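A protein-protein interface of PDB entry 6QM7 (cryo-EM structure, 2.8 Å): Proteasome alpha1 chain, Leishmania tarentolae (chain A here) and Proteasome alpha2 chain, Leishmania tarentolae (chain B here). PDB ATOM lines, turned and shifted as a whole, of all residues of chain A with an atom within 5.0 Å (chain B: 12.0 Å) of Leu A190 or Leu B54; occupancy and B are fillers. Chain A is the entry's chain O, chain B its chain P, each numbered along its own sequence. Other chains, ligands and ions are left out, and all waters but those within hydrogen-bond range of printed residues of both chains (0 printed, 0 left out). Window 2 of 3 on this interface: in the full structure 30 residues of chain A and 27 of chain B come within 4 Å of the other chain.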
ATOM      1  N   ILE A  39       6.443 -24.006  13.415  1.00  0.00           N
ATOM      2  CA  ILE A  39       5.437 -23.596  14.425  1.00  0.00           C
ATOM      3  C   ILE A  39       4.143 -24.367  14.179  1.00  0.00           C
ATOM      4  O   ILE A  39       3.785 -24.675  13.041  1.00  0.00           O
ATOM      5  CB  ILE A  39       5.223 -22.079  14.392  1.00  0.00           C
ATOM      6  CG1 ILE A  39       4.449 -21.590  15.617  1.00  0.00           C
ATOM      7  CG2 ILE A  39       4.549 -21.665  13.099  1.00  0.00           C
ATOM      8  CD1 ILE A  39       4.663 -20.125  15.914  1.00  0.00           C
ATOM      9  N   ARG A  40       3.482 -24.655  15.273  1.00  0.00           N
ATOM     10  CA  ARG A  40       2.312 -25.532  15.373  1.00  0.00           C
ATOM     11  C   ARG A  40       1.212 -24.603  15.858  1.00  0.00           C
ATOM     12  O   ARG A  40       1.462 -23.873  16.817  1.00  0.00           O
ATOM     13  CB  ARG A  40       2.730 -26.632  16.346  1.00  0.00           C
ATOM     14  CG  ARG A  40       1.679 -27.678  16.620  1.00  0.00           C
ATOM     15  CD  ARG A  40       1.447 -27.779  18.109  1.00  0.00           C
ATOM     16  NE  ARG A  40       2.239 -28.788  18.779  1.00  0.00           N
ATOM     17  CZ  ARG A  40       2.113 -29.083  20.063  1.00  0.00           C
ATOM     18  NH1 ARG A  40       2.849 -30.038  20.591  1.00  0.00           N
ATOM     19  NH2 ARG A  40       1.249 -28.441  20.829  1.00  0.00           N
ATOM     20  N   CYS A  41       0.101 -24.523  15.151  1.00  0.00           N
ATOM     21  CA  CYS A  41      -1.035 -23.657  15.537  1.00  0.00           C
ATOM     22  C   CYS A  41      -2.177 -24.579  15.973  1.00  0.00           C
ATOM     23  O   CYS A  41      -1.893 -25.749  16.314  1.00  0.00           O
ATOM     24  CB  CYS A  41      -1.366 -22.705  14.396  1.00  0.00           C
ATOM     25  SG  CYS A  41      -2.184 -23.496  12.988  1.00  0.00           S
ATOM     26  N   HIS A 165       7.693 -30.511  19.583  1.00  0.00           N
ATOM     27  CA  HIS A 165       7.837 -29.049  19.769  1.00  0.00           C
ATOM     28  C   HIS A 165       6.499 -28.373  19.526  1.00  0.00           C
ATOM     29  O   HIS A 165       5.696 -28.917  18.755  1.00  0.00           O
ATOM     30  CB  HIS A 165       8.912 -28.473  18.850  1.00  0.00           C
ATOM     31  CG  HIS A 165      10.259 -29.009  19.152  1.00  0.00           C
ATOM     32  ND1 HIS A 165      11.083 -28.430  20.087  1.00  0.00           N
ATOM     33  CD2 HIS A 165      10.913 -30.078  18.658  1.00  0.00           C
ATOM     34  CE1 HIS A 165      12.206 -29.122  20.152  1.00  0.00           C
ATOM     35  NE2 HIS A 165      12.128 -30.140  19.282  1.00  0.00           N
ATOM     36  N   ILE A 166       6.309 -27.235  20.185  1.00  0.00           N
ATOM     37  CA  ILE A 166       5.243 -26.252  19.870  1.00  0.00           C
ATOM     38  C   ILE A 166       5.802 -25.337  18.778  1.00  0.00           C
ATOM     39  O   ILE A 166       5.121 -25.152  17.749  1.00  0.00           O
ATOM     40  CB  ILE A 166       4.809 -25.501  21.139  1.00  0.00           C
ATOM     41  CG1 ILE A 166       4.149 -26.449  22.141  1.00  0.00           C
ATOM     42  CG2 ILE A 166       3.901 -24.336  20.792  1.00  0.00           C
ATOM     43  CD1 ILE A 166       4.223 -25.963  23.575  1.00  0.00           C
ATOM     44  N   ALA A 167       7.001 -24.797  18.989  1.00  0.00           N
ATOM     45  CA  ALA A 167       7.794 -24.116  17.941  1.00  0.00           C
ATOM     46  C   ALA A 167       9.248 -24.522  18.105  1.00  0.00           C
ATOM     47  O   ALA A 167       9.655 -24.841  19.228  1.00  0.00           O
ATOM     48  CB  ALA A 167       7.631 -22.620  18.010  1.00  0.00           C
ATOM     49  N   MET A 178      14.669 -18.732  18.775  1.00  0.00           N
ATOM     50  CA  MET A 178      13.984 -19.339  19.946  1.00  0.00           C
ATOM     51  C   MET A 178      13.639 -18.231  20.941  1.00  0.00           C
ATOM     52  O   MET A 178      12.468 -18.152  21.327  1.00  0.00           O
ATOM     53  CB  MET A 178      14.853 -20.396  20.638  1.00  0.00           C
ATOM     54  CG  MET A 178      14.929 -21.725  19.895  1.00  0.00           C
ATOM     55  SD  MET A 178      13.335 -22.568  19.780  1.00  0.00           S
ATOM     56  CE  MET A 178      13.852 -24.281  19.929  1.00  0.00           C
ATOM     57  N   LEU A 181      10.532 -16.490  19.785  1.00  0.00           N
ATOM     58  CA  LEU A 181       9.354 -17.388  19.933  1.00  0.00           C
ATOM     59  C   LEU A 181       8.999 -17.596  21.415  1.00  0.00           C
ATOM     60  O   LEU A 181       7.797 -17.717  21.704  1.00  0.00           O
ATOM     61  CB  LEU A 181       9.665 -18.727  19.262  1.00  0.00           C
ATOM     62  CG  LEU A 181       9.752 -18.689  17.738  1.00  0.00           C
ATOM     63  CD1 LEU A 181      10.565 -19.865  17.193  1.00  0.00           C
ATOM     64  CD2 LEU A 181       8.355 -18.665  17.134  1.00  0.00           C
ATOM     65  N   GLU A 182       9.993 -17.673  22.312  1.00  0.00           N
ATOM     66  CA  GLU A 182       9.801 -17.846  23.783  1.00  0.00           C
ATOM     67  C   GLU A 182       9.177 -16.578  24.370  1.00  0.00           C
ATOM     68  O   GLU A 182       8.348 -16.717  25.280  1.00  0.00           O
ATOM     69  CB  GLU A 182      11.120 -18.134  24.509  1.00  0.00           C
ATOM     70  CG  GLU A 182      11.643 -19.548  24.319  1.00  0.00           C
ATOM     71  CD  GLU A 182      13.106 -19.760  24.698  1.00  0.00           C
ATOM     72  OE1 GLU A 182      13.748 -20.669  24.118  1.00  0.00           O
ATOM     73  OE2 GLU A 182      13.609 -19.015  25.570  1.00  0.00           O
ATOM     74  N   ARG A 184       7.341 -14.500  22.638  1.00  0.00           N
ATOM     75  CA  ARG A 184       5.998 -14.435  22.000  1.00  0.00           C
ATOM     76  C   ARG A 184       5.063 -15.495  22.594  1.00  0.00           C
ATOM     77  O   ARG A 184       3.855 -15.392  22.338  1.00  0.00           O
ATOM     78  CB  ARG A 184       6.118 -14.604  20.481  1.00  0.00           C
ATOM     79  CG  ARG A 184       5.190 -13.706  19.676  1.00  0.00           C
ATOM     80  CD  ARG A 184       5.476 -12.219  19.856  1.00  0.00           C
ATOM     81  NE  ARG A 184       5.797 -11.525  18.611  1.00  0.00           N
ATOM     82  CZ  ARG A 184       4.990 -11.410  17.552  1.00  0.00           C
ATOM     83  NH1 ARG A 184       3.782 -11.959  17.550  1.00  0.00           N
ATOM     84  NH2 ARG A 184       5.405 -10.746  16.483  1.00  0.00           N
ATOM     85  N   GLN A 185       5.589 -16.471  23.341  1.00  0.00           N
ATOM     86  CA  GLN A 185       4.804 -17.558  23.989  1.00  0.00           C
ATOM     87  C   GLN A 185       4.247 -17.092  25.344  1.00  0.00           C
ATOM     88  O   GLN A 185       3.272 -17.706  25.805  1.00  0.00           O
ATOM     89  CB  GLN A 185       5.670 -18.805  24.176  1.00  0.00           C
ATOM     90  CG  GLN A 185       4.866 -20.082  24.386  1.00  0.00           C
ATOM     91  CD  GLN A 185       5.724 -21.251  24.794  1.00  0.00           C
ATOM     92  OE1 GLN A 185       6.882 -21.098  25.179  1.00  0.00           O
ATOM     93  NE2 GLN A 185       5.149 -22.441  24.709  1.00  0.00           N
ATOM     94  N   THR A 188       0.850 -14.835  24.048  1.00  0.00           N
ATOM     95  CA  THR A 188      -0.231 -15.630  23.395  1.00  0.00           C
ATOM     96  C   THR A 188      -0.150 -17.087  23.878  1.00  0.00           C
ATOM     97  O   THR A 188       0.854 -17.435  24.523  1.00  0.00           O
ATOM     98  CB  THR A 188      -0.139 -15.493  21.866  1.00  0.00           C
ATOM     99  OG1 THR A 188       1.140 -15.947  21.420  1.00  0.00           O
ATOM    100  CG2 THR A 188      -0.334 -14.073  21.377  1.00  0.00           C
ATOM    101  N   GLU A 189      -1.175 -17.899  23.593  1.00  0.00           N
ATOM    102  CA  GLU A 189      -1.221 -19.346  23.954  1.00  0.00           C
ATOM    103  C   GLU A 189      -0.296 -20.128  23.013  1.00  0.00           C
ATOM    104  O   GLU A 189       0.420 -21.017  23.513  1.00  0.00           O
ATOM    105  CB  GLU A 189      -2.646 -19.903  23.889  1.00  0.00           C
ATOM    106  CG  GLU A 189      -3.528 -19.491  25.063  1.00  0.00           C
ATOM    107  CD  GLU A 189      -4.949 -20.039  25.028  1.00  0.00           C
ATOM    108  OE1 GLU A 189      -5.111 -21.259  24.816  1.00  0.00           O
ATOM    109  OE2 GLU A 189      -5.897 -19.244  25.207  1.00  0.00           O
ATOM    110  N   LEU A 190      -0.356 -19.827  21.707  1.00  0.00           N
ATOM    111  CA  LEU A 190       0.511 -20.347  20.601  1.00  0.00           C
ATOM    112  C   LEU A 190      -0.084 -21.628  19.996  1.00  0.00           C
ATOM    113  O   LEU A 190       0.220 -21.900  18.827  1.00  0.00           O
ATOM    114  CB  LEU A 190       1.962 -20.550  21.068  1.00  0.00           C
ATOM    115  CG  LEU A 190       3.035 -20.085  20.077  1.00  0.00           C
ATOM    116  CD1 LEU A 190       3.075 -18.567  19.984  1.00  0.00           C
ATOM    117  CD2 LEU A 190       4.416 -20.606  20.447  1.00  0.00           C
ATOM    118  N   ASP A 191      -0.911 -22.363  20.750  1.00  0.00           N
ATOM    119  CA  ASP A 191      -1.701 -23.535  20.278  1.00  0.00           C
ATOM    120  C   ASP A 191      -3.159 -23.132  20.019  1.00  0.00           C
ATOM    121  O   ASP A 191      -3.920 -23.988  19.517  1.00  0.00           O
ATOM    122  CB  ASP A 191      -1.662 -24.680  21.300  1.00  0.00           C
ATOM    123  CG  ASP A 191      -0.431 -25.563  21.207  1.00  0.00           C
ATOM    124  OD1 ASP A 191      -0.112 -25.997  20.079  1.00  0.00           O
ATOM    125  OD2 ASP A 191       0.198 -25.812  22.260  1.00  0.00           O
ATOM    126  N   ALA A 192      -3.547 -21.902  20.381  1.00  0.00           N
ATOM    127  CA  ALA A 192      -4.896 -21.331  20.154  1.00  0.00           C
ATOM    128  C   ALA A 192      -4.864 -20.374  18.957  1.00  0.00           C
ATOM    129  O   ALA A 192      -5.893 -19.722  18.693  1.00  0.00           O
ATOM    130  CB  ALA A 192      -5.362 -20.637  21.407  1.00  0.00           C
ATOM    131  N   LEU A 193      -3.736 -20.321  18.245  1.00  0.00           N
ATOM    132  CA  LEU A 193      -3.482 -19.359  17.144  1.00  0.00           C
ATOM    133  C   LEU A 193      -4.074 -19.889  15.837  1.00  0.00           C
ATOM    134  O   LEU A 193      -4.202 -21.116  15.691  1.00  0.00           O
ATOM    135  CB  LEU A 193      -1.971 -19.121  17.018  1.00  0.00           C
ATOM    136  CG  LEU A 193      -1.493 -17.722  17.411  1.00  0.00           C
ATOM    137  CD1 LEU A 193      -2.077 -17.266  18.746  1.00  0.00           C
ATOM    138  CD2 LEU A 193       0.027 -17.672  17.439  1.00  0.00           C
ATOM    139  N   ILE A 201       4.251 -15.126  13.203  1.00  0.00           N
ATOM    140  CA  ILE A 201       5.206 -15.332  14.332  1.00  0.00           C
ATOM    141  C   ILE A 201       6.448 -16.049  13.804  1.00  0.00           C
ATOM    142  O   ILE A 201       7.560 -15.603  14.124  1.00  0.00           O
ATOM    143  CB  ILE A 201       4.560 -16.106  15.495  1.00  0.00           C
ATOM    144  CG1 ILE A 201       3.436 -15.280  16.131  1.00  0.00           C
ATOM    145  CG2 ILE A 201       5.620 -16.532  16.505  1.00  0.00           C
ATOM    146  CD1 ILE A 201       2.959 -15.773  17.477  1.00  0.00           C
ATOM    147  N   LYS B  48      12.011 -33.870  34.069  1.00  0.00           N
ATOM    148  CA  LYS B  48      12.128 -33.692  32.597  1.00  0.00           C
ATOM    149  C   LYS B  48      12.187 -32.192  32.305  1.00  0.00           C
ATOM    150  O   LYS B  48      11.303 -31.686  31.592  1.00  0.00           O
ATOM    151  CB  LYS B  48      10.987 -34.401  31.853  1.00  0.00           C
ATOM    152  CG  LYS B  48       9.575 -34.089  32.328  1.00  0.00           C
ATOM    153  CD  LYS B  48       8.517 -34.130  31.241  1.00  0.00           C
ATOM    154  CE  LYS B  48       8.019 -35.523  30.932  1.00  0.00           C
ATOM    155  NZ  LYS B  48       6.600 -35.492  30.508  1.00  0.00           N
ATOM    156  N   LYS B  49      13.187 -31.517  32.882  1.00  0.00           N
ATOM    157  CA  LYS B  49      13.572 -30.116  32.558  1.00  0.00           C
ATOM    158  C   LYS B  49      13.768 -30.022  31.039  1.00  0.00           C
ATOM    159  O   LYS B  49      14.731 -30.635  30.528  1.00  0.00           O
ATOM    160  CB  LYS B  49      14.830 -29.735  33.353  1.00  0.00           C
ATOM    161  CG  LYS B  49      15.561 -28.460  32.932  1.00  0.00           C
ATOM    162  CD  LYS B  49      17.033 -28.450  33.329  1.00  0.00           C
ATOM    163  CE  LYS B  49      17.908 -29.345  32.470  1.00  0.00           C
ATOM    164  NZ  LYS B  49      18.423 -28.637  31.274  1.00  0.00           N
ATOM    165  N   ALA B  50      12.869 -29.308  30.353  1.00  0.00           N
ATOM    166  CA  ALA B  50      12.896 -29.093  28.888  1.00  0.00           C
ATOM    167  C   ALA B  50      13.828 -27.925  28.563  1.00  0.00           C
ATOM    168  O   ALA B  50      13.843 -26.934  29.291  1.00  0.00           O
ATOM    169  CB  ALA B  50      11.494 -28.843  28.389  1.00  0.00           C
ATOM    170  N   PRO B  51      14.633 -27.997  27.471  1.00  0.00           N
ATOM    171  CA  PRO B  51      15.509 -26.887  27.084  1.00  0.00           C
ATOM    172  C   PRO B  51      14.806 -25.521  27.135  1.00  0.00           C
ATOM    173  O   PRO B  51      15.335 -24.623  27.762  1.00  0.00           O
ATOM    174  CB  PRO B  51      15.919 -27.233  25.641  1.00  0.00           C
ATOM    175  CG  PRO B  51      15.833 -28.751  25.571  1.00  0.00           C
ATOM    176  CD  PRO B  51      14.755 -29.149  26.560  1.00  0.00           C
ATOM    177  N   SER B  52      13.633 -25.420  26.496  1.00  0.00           N
ATOM    178  CA  SER B  52      12.775 -24.207  26.420  1.00  0.00           C
ATOM    179  C   SER B  52      11.318 -24.576  26.697  1.00  0.00           C
ATOM    180  O   SER B  52      10.997 -25.771  26.699  1.00  0.00           O
ATOM    181  CB  SER B  52      12.903 -23.522  25.079  1.00  0.00           C
ATOM    182  OG  SER B  52      12.556 -24.393  24.013  1.00  0.00           O
ATOM    183  N   THR B  53      10.475 -23.559  26.876  1.00  0.00           N
ATOM    184  CA  THR B  53       9.010 -23.674  27.101  1.00  0.00           C
ATOM    185  C   THR B  53       8.309 -24.061  25.793  1.00  0.00           C
ATOM    186  O   THR B  53       7.107 -24.416  25.850  1.00  0.00           O
ATOM    187  CB  THR B  53       8.463 -22.365  27.680  1.00  0.00           C
ATOM    188  OG1 THR B  53       8.863 -21.294  26.821  1.00  0.00           O
ATOM    189  CG2 THR B  53       8.963 -22.101  29.085  1.00  0.00           C
ATOM    190  N   LEU B  54       9.028 -23.989  24.667  1.00  0.00           N
ATOM    191  CA  LEU B  54       8.526 -24.310  23.303  1.00  0.00           C
ATOM    192  C   LEU B  54       8.530 -25.813  23.031  1.00  0.00           C
ATOM    193  O   LEU B  54       7.938 -26.213  22.019  1.00  0.00           O
ATOM    194  CB  LEU B  54       9.400 -23.594  22.276  1.00  0.00           C
ATOM    195  CG  LEU B  54       9.277 -22.076  22.281  1.00  0.00           C
ATOM    196  CD1 LEU B  54      10.309 -21.458  21.357  1.00  0.00           C
ATOM    197  CD2 LEU B  54       7.875 -21.645  21.881  1.00  0.00           C
ATOM    198  N   VAL B  55       9.171 -26.618  23.870  1.00  0.00           N
ATOM    199  CA  VAL B  55       9.142 -28.100  23.725  1.00  0.00           C
ATOM    200  C   VAL B  55       7.793 -28.590  24.240  1.00  0.00           C
ATOM    201  O   VAL B  55       7.398 -28.165  25.340  1.00  0.00           O
ATOM    202  CB  VAL B  55      10.317 -28.776  24.453  1.00  0.00           C
ATOM    203  CG1 VAL B  55      10.291 -30.285  24.278  1.00  0.00           C
ATOM    204  CG2 VAL B  55      11.651 -28.209  23.982  1.00  0.00           C
ATOM    205  N   ASP B  56       7.116 -29.431  23.455  1.00  0.00           N
ATOM    206  CA  ASP B  56       5.876 -30.127  23.873  1.00  0.00           C
ATOM    207  C   ASP B  56       6.278 -31.082  24.997  1.00  0.00           C
ATOM    208  O   ASP B  56       6.808 -32.163  24.681  1.00  0.00           O
ATOM    209  CB  ASP B  56       5.208 -30.866  22.710  1.00  0.00           C
ATOM    210  CG  ASP B  56       3.903 -31.572  23.068  1.00  0.00           C
ATOM    211  OD1 ASP B  56       3.377 -31.332  24.181  1.00  0.00           O
ATOM    212  OD2 ASP B  56       3.393 -32.337  22.213  1.00  0.00           O
ATOM    213  N   ALA B  57       6.082 -30.662  26.250  1.00  0.00           N
ATOM    214  CA  ALA B  57       6.492 -31.401  27.463  1.00  0.00           C
ATOM    215  C   ALA B  57       6.010 -32.856  27.381  1.00  0.00           C
ATOM    216  O   ALA B  57       6.790 -33.754  27.732  1.00  0.00           O
ATOM    217  CB  ALA B  57       5.947 -30.705  28.680  1.00  0.00           C
ATOM    218  N   SER B  58       4.785 -33.085  26.906  1.00  0.00           N
ATOM    219  CA  SER B  58       4.164 -34.432  26.789  1.00  0.00           C
ATOM    220  C   SER B  58       4.972 -35.339  25.852  1.00  0.00           C
ATOM    221  O   SER B  58       4.874 -36.556  26.017  1.00  0.00           O
ATOM    222  CB  SER B  58       2.731 -34.338  26.338  1.00  0.00           C
ATOM    223  OG  SER B  58       2.640 -33.722  25.065  1.00  0.00           O
ATOM    224  N   SER B  59       5.705 -34.789  24.883  1.00  0.00           N
ATOM    225  CA  SER B  59       6.551 -35.551  23.918  1.00  0.00           C
ATOM    226  C   SER B  59       7.863 -35.999  24.574  1.00  0.00           C
ATOM    227  O   SER B  59       8.503 -36.902  24.020  1.00  0.00           O
ATOM    228  CB  SER B  59       6.845 -34.742  22.680  1.00  0.00           C
ATOM    229  OG  SER B  59       7.951 -33.868  22.894  1.00  0.00           O
ATOM    230  N   ILE B  60       8.283 -35.337  25.659  1.00  0.00           N
ATOM    231  CA  ILE B  60       9.446 -35.771  26.484  1.00  0.00           C
ATOM    232  C   ILE B  60       8.961 -36.933  27.346  1.00  0.00           C
ATOM    233  O   ILE B  60       7.826 -36.883  27.854  1.00  0.00           O
ATOM    234  CB  ILE B  60      10.045 -34.660  27.360  1.00  0.00           C
ATOM    235  CG1 ILE B  60      10.370 -33.387  26.574  1.00  0.00           C
ATOM    236  CG2 ILE B  60      11.271 -35.186  28.099  1.00  0.00           C
ATOM    237  CD1 ILE B  60      10.526 -32.153  27.457  1.00  0.00           C
ATOM    238  N   GLU B 204       4.131 -31.022  34.177  1.00  0.00           N
ATOM    239  CA  GLU B 204       4.865 -30.837  32.895  1.00  0.00           C
ATOM    240  C   GLU B 204       6.371 -30.995  33.133  1.00  0.00           C
ATOM    241  O   GLU B 204       7.089 -31.324  32.173  1.00  0.00           O
ATOM    242  CB  GLU B 204       4.579 -29.451  32.298  1.00  0.00           C
ATOM    243  CG  GLU B 204       3.126 -29.232  31.882  1.00  0.00           C
ATOM    244  CD  GLU B 204       2.177 -28.766  32.979  1.00  0.00           C
ATOM    245  OE1 GLU B 204       1.684 -29.625  33.736  1.00  0.00           O
ATOM    246  OE2 GLU B 204       1.937 -27.543  33.079  1.00  0.00           O
ATOM    247  N   ASN B 205       6.820 -30.744  34.362  1.00  0.00           N
ATOM    248  CA  ASN B 205       8.249 -30.562  34.737  1.00  0.00           C
ATOM    249  C   ASN B 205       8.859 -31.897  35.189  1.00  0.00           C
ATOM    250  O   ASN B 205      10.072 -32.083  34.984  1.00  0.00           O
ATOM    251  CB  ASN B 205       8.359 -29.539  35.868  1.00  0.00           C
ATOM    252  CG  ASN B 205       9.603 -28.688  35.821  1.00  0.00           C
ATOM    253  OD1 ASN B 205      10.566 -29.001  35.121  1.00  0.00           O
ATOM    254  ND2 ASN B 205       9.588 -27.608  36.585  1.00  0.00           N
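NE of Arg A40 sits at hydrogen-bond distance from O of His A165, 3.5 Å away.
O of Ile A166 is in hydrogen-bond range of N of Arg A40 (3.0 Å).
The guanidinium group (NH2) of Arg A40 is in salt-bridge range of the side-chain carboxylate (OD1) of Asp A191, 2.9 Å away.
OD1 of Asp B56 sits at hydrogen-bond distance from OG of Ser B58 (2.7 Å).
The backbone carbonyl oxygen (O) of Asp B56 lies within hydrogen-bond range of the side-chain hydroxyl (OG) of Ser B59.
Along chain B the printed residues that touch a printed residue of chain A span positions 52 to 56.
Of the 18 printed residues of chain A, 9 touch a printed residue of chain B.
Hydrophobic or aromatic side chains of chain A that line the printed part of chain B: His A165, Ile A166, Ala A167, Met A178, Leu A181 and Leu A190.
Among the printed residues, 14 pairs touch across the chains.
Printed residues of chain B within 4 Å of Leu A190: Leu B54.
Of the printed residues of chain A, Leu B54 touches His A165 (3.6 Å), Ile A166 (2.7 Å), Ala A167 (3.3 Å), Met A178 (3.6 Å), Leu A181 (3.5 Å), Glu A182 (3.8 Å), Gln A185 (3.5 Å) and Leu A190 (3.9 Å).
No residue of chain B comes within 4 Å of Cys A41.
Printed residues of chain B within 4 Å of Ala A167: Leu B54 (3.3 Å).
Of chain B, only Leu B54 (3.6 Å) comes within 4 Å of Met A178.
Printed residues of chain B within 4 Å of Leu A181: Leu B54.
No residue of chain B comes within 4 Å of Thr A188.
Glu A189 touches none of the printed residues of chain B.
Asp A191 touches none of the printed residues of chain B.
Of the printed residues of chain A, Asp B56 touches Arg A40 (2.9 Å) and His A165 (3.8 Å).
Of the printed residues of chain A, Val B55 touches His A165 (3.9 Å).
Printed residues of chain A within 4 Å of Thr B53: Ile A166 (3.99 Å) and Gln A185 (2.6 Å).
Of the printed residues of chain B, Ile A166 touches Thr B53 (3.99 Å) and Leu B54 (2.7 Å).
Of the printed residues of chain A, Ser B52 touches Glu A182.
Lys B48 touches none of the printed residues of chain A.
The nearest residue of chain B that does not touch Leu A190 is Thr B53 (7.1 Å).
The nearest printed residue of chain A that does not touch Leu B54 is Arg A40 (6.5 Å).
The nearest printed residue of chain A that does not touch Ser B52 is Met A178 (4.3 Å).
Among the printed residues, pairs that only touch across the chains: His A165 with Leu B54 (3.6 Å), His A165 with Val B55 (3.9 Å), His A165 with Asp B56 (3.8 Å), Ile A166 with Thr B53 (3.99 Å), Met A178 with Leu B54 (3.6 Å), Leu A181 with Leu B54 (3.5 Å), Glu A182 with Ser B52 (3.1 Å), Glu A182 with Leu B54 (3.8 Å), Gln A185 with Leu B54 (3.5 Å) and Leu A190 with Leu B54 (3.9 Å).
The guanidinium group (NH1) of Arg A40 is in salt-bridge range of the side-chain carboxylate (OD2) of Asp B56, 2.9 Å away.
The backbone carbonyl oxygen (O) of Leu B54 lies within hydrogen-bond range of the backbone NH (N) of Ile A166 (2.7 Å).
The backbone NH (N) of Ala A167 lies within hydrogen-bond range of the backbone carbonyl oxygen (O) of Leu B54 (3.5 Å).
The side-chain amide oxygen of Gln A185 sits at hydrogen-bond distance from the side-chain hydroxyl of Thr B53 (2.6 Å).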
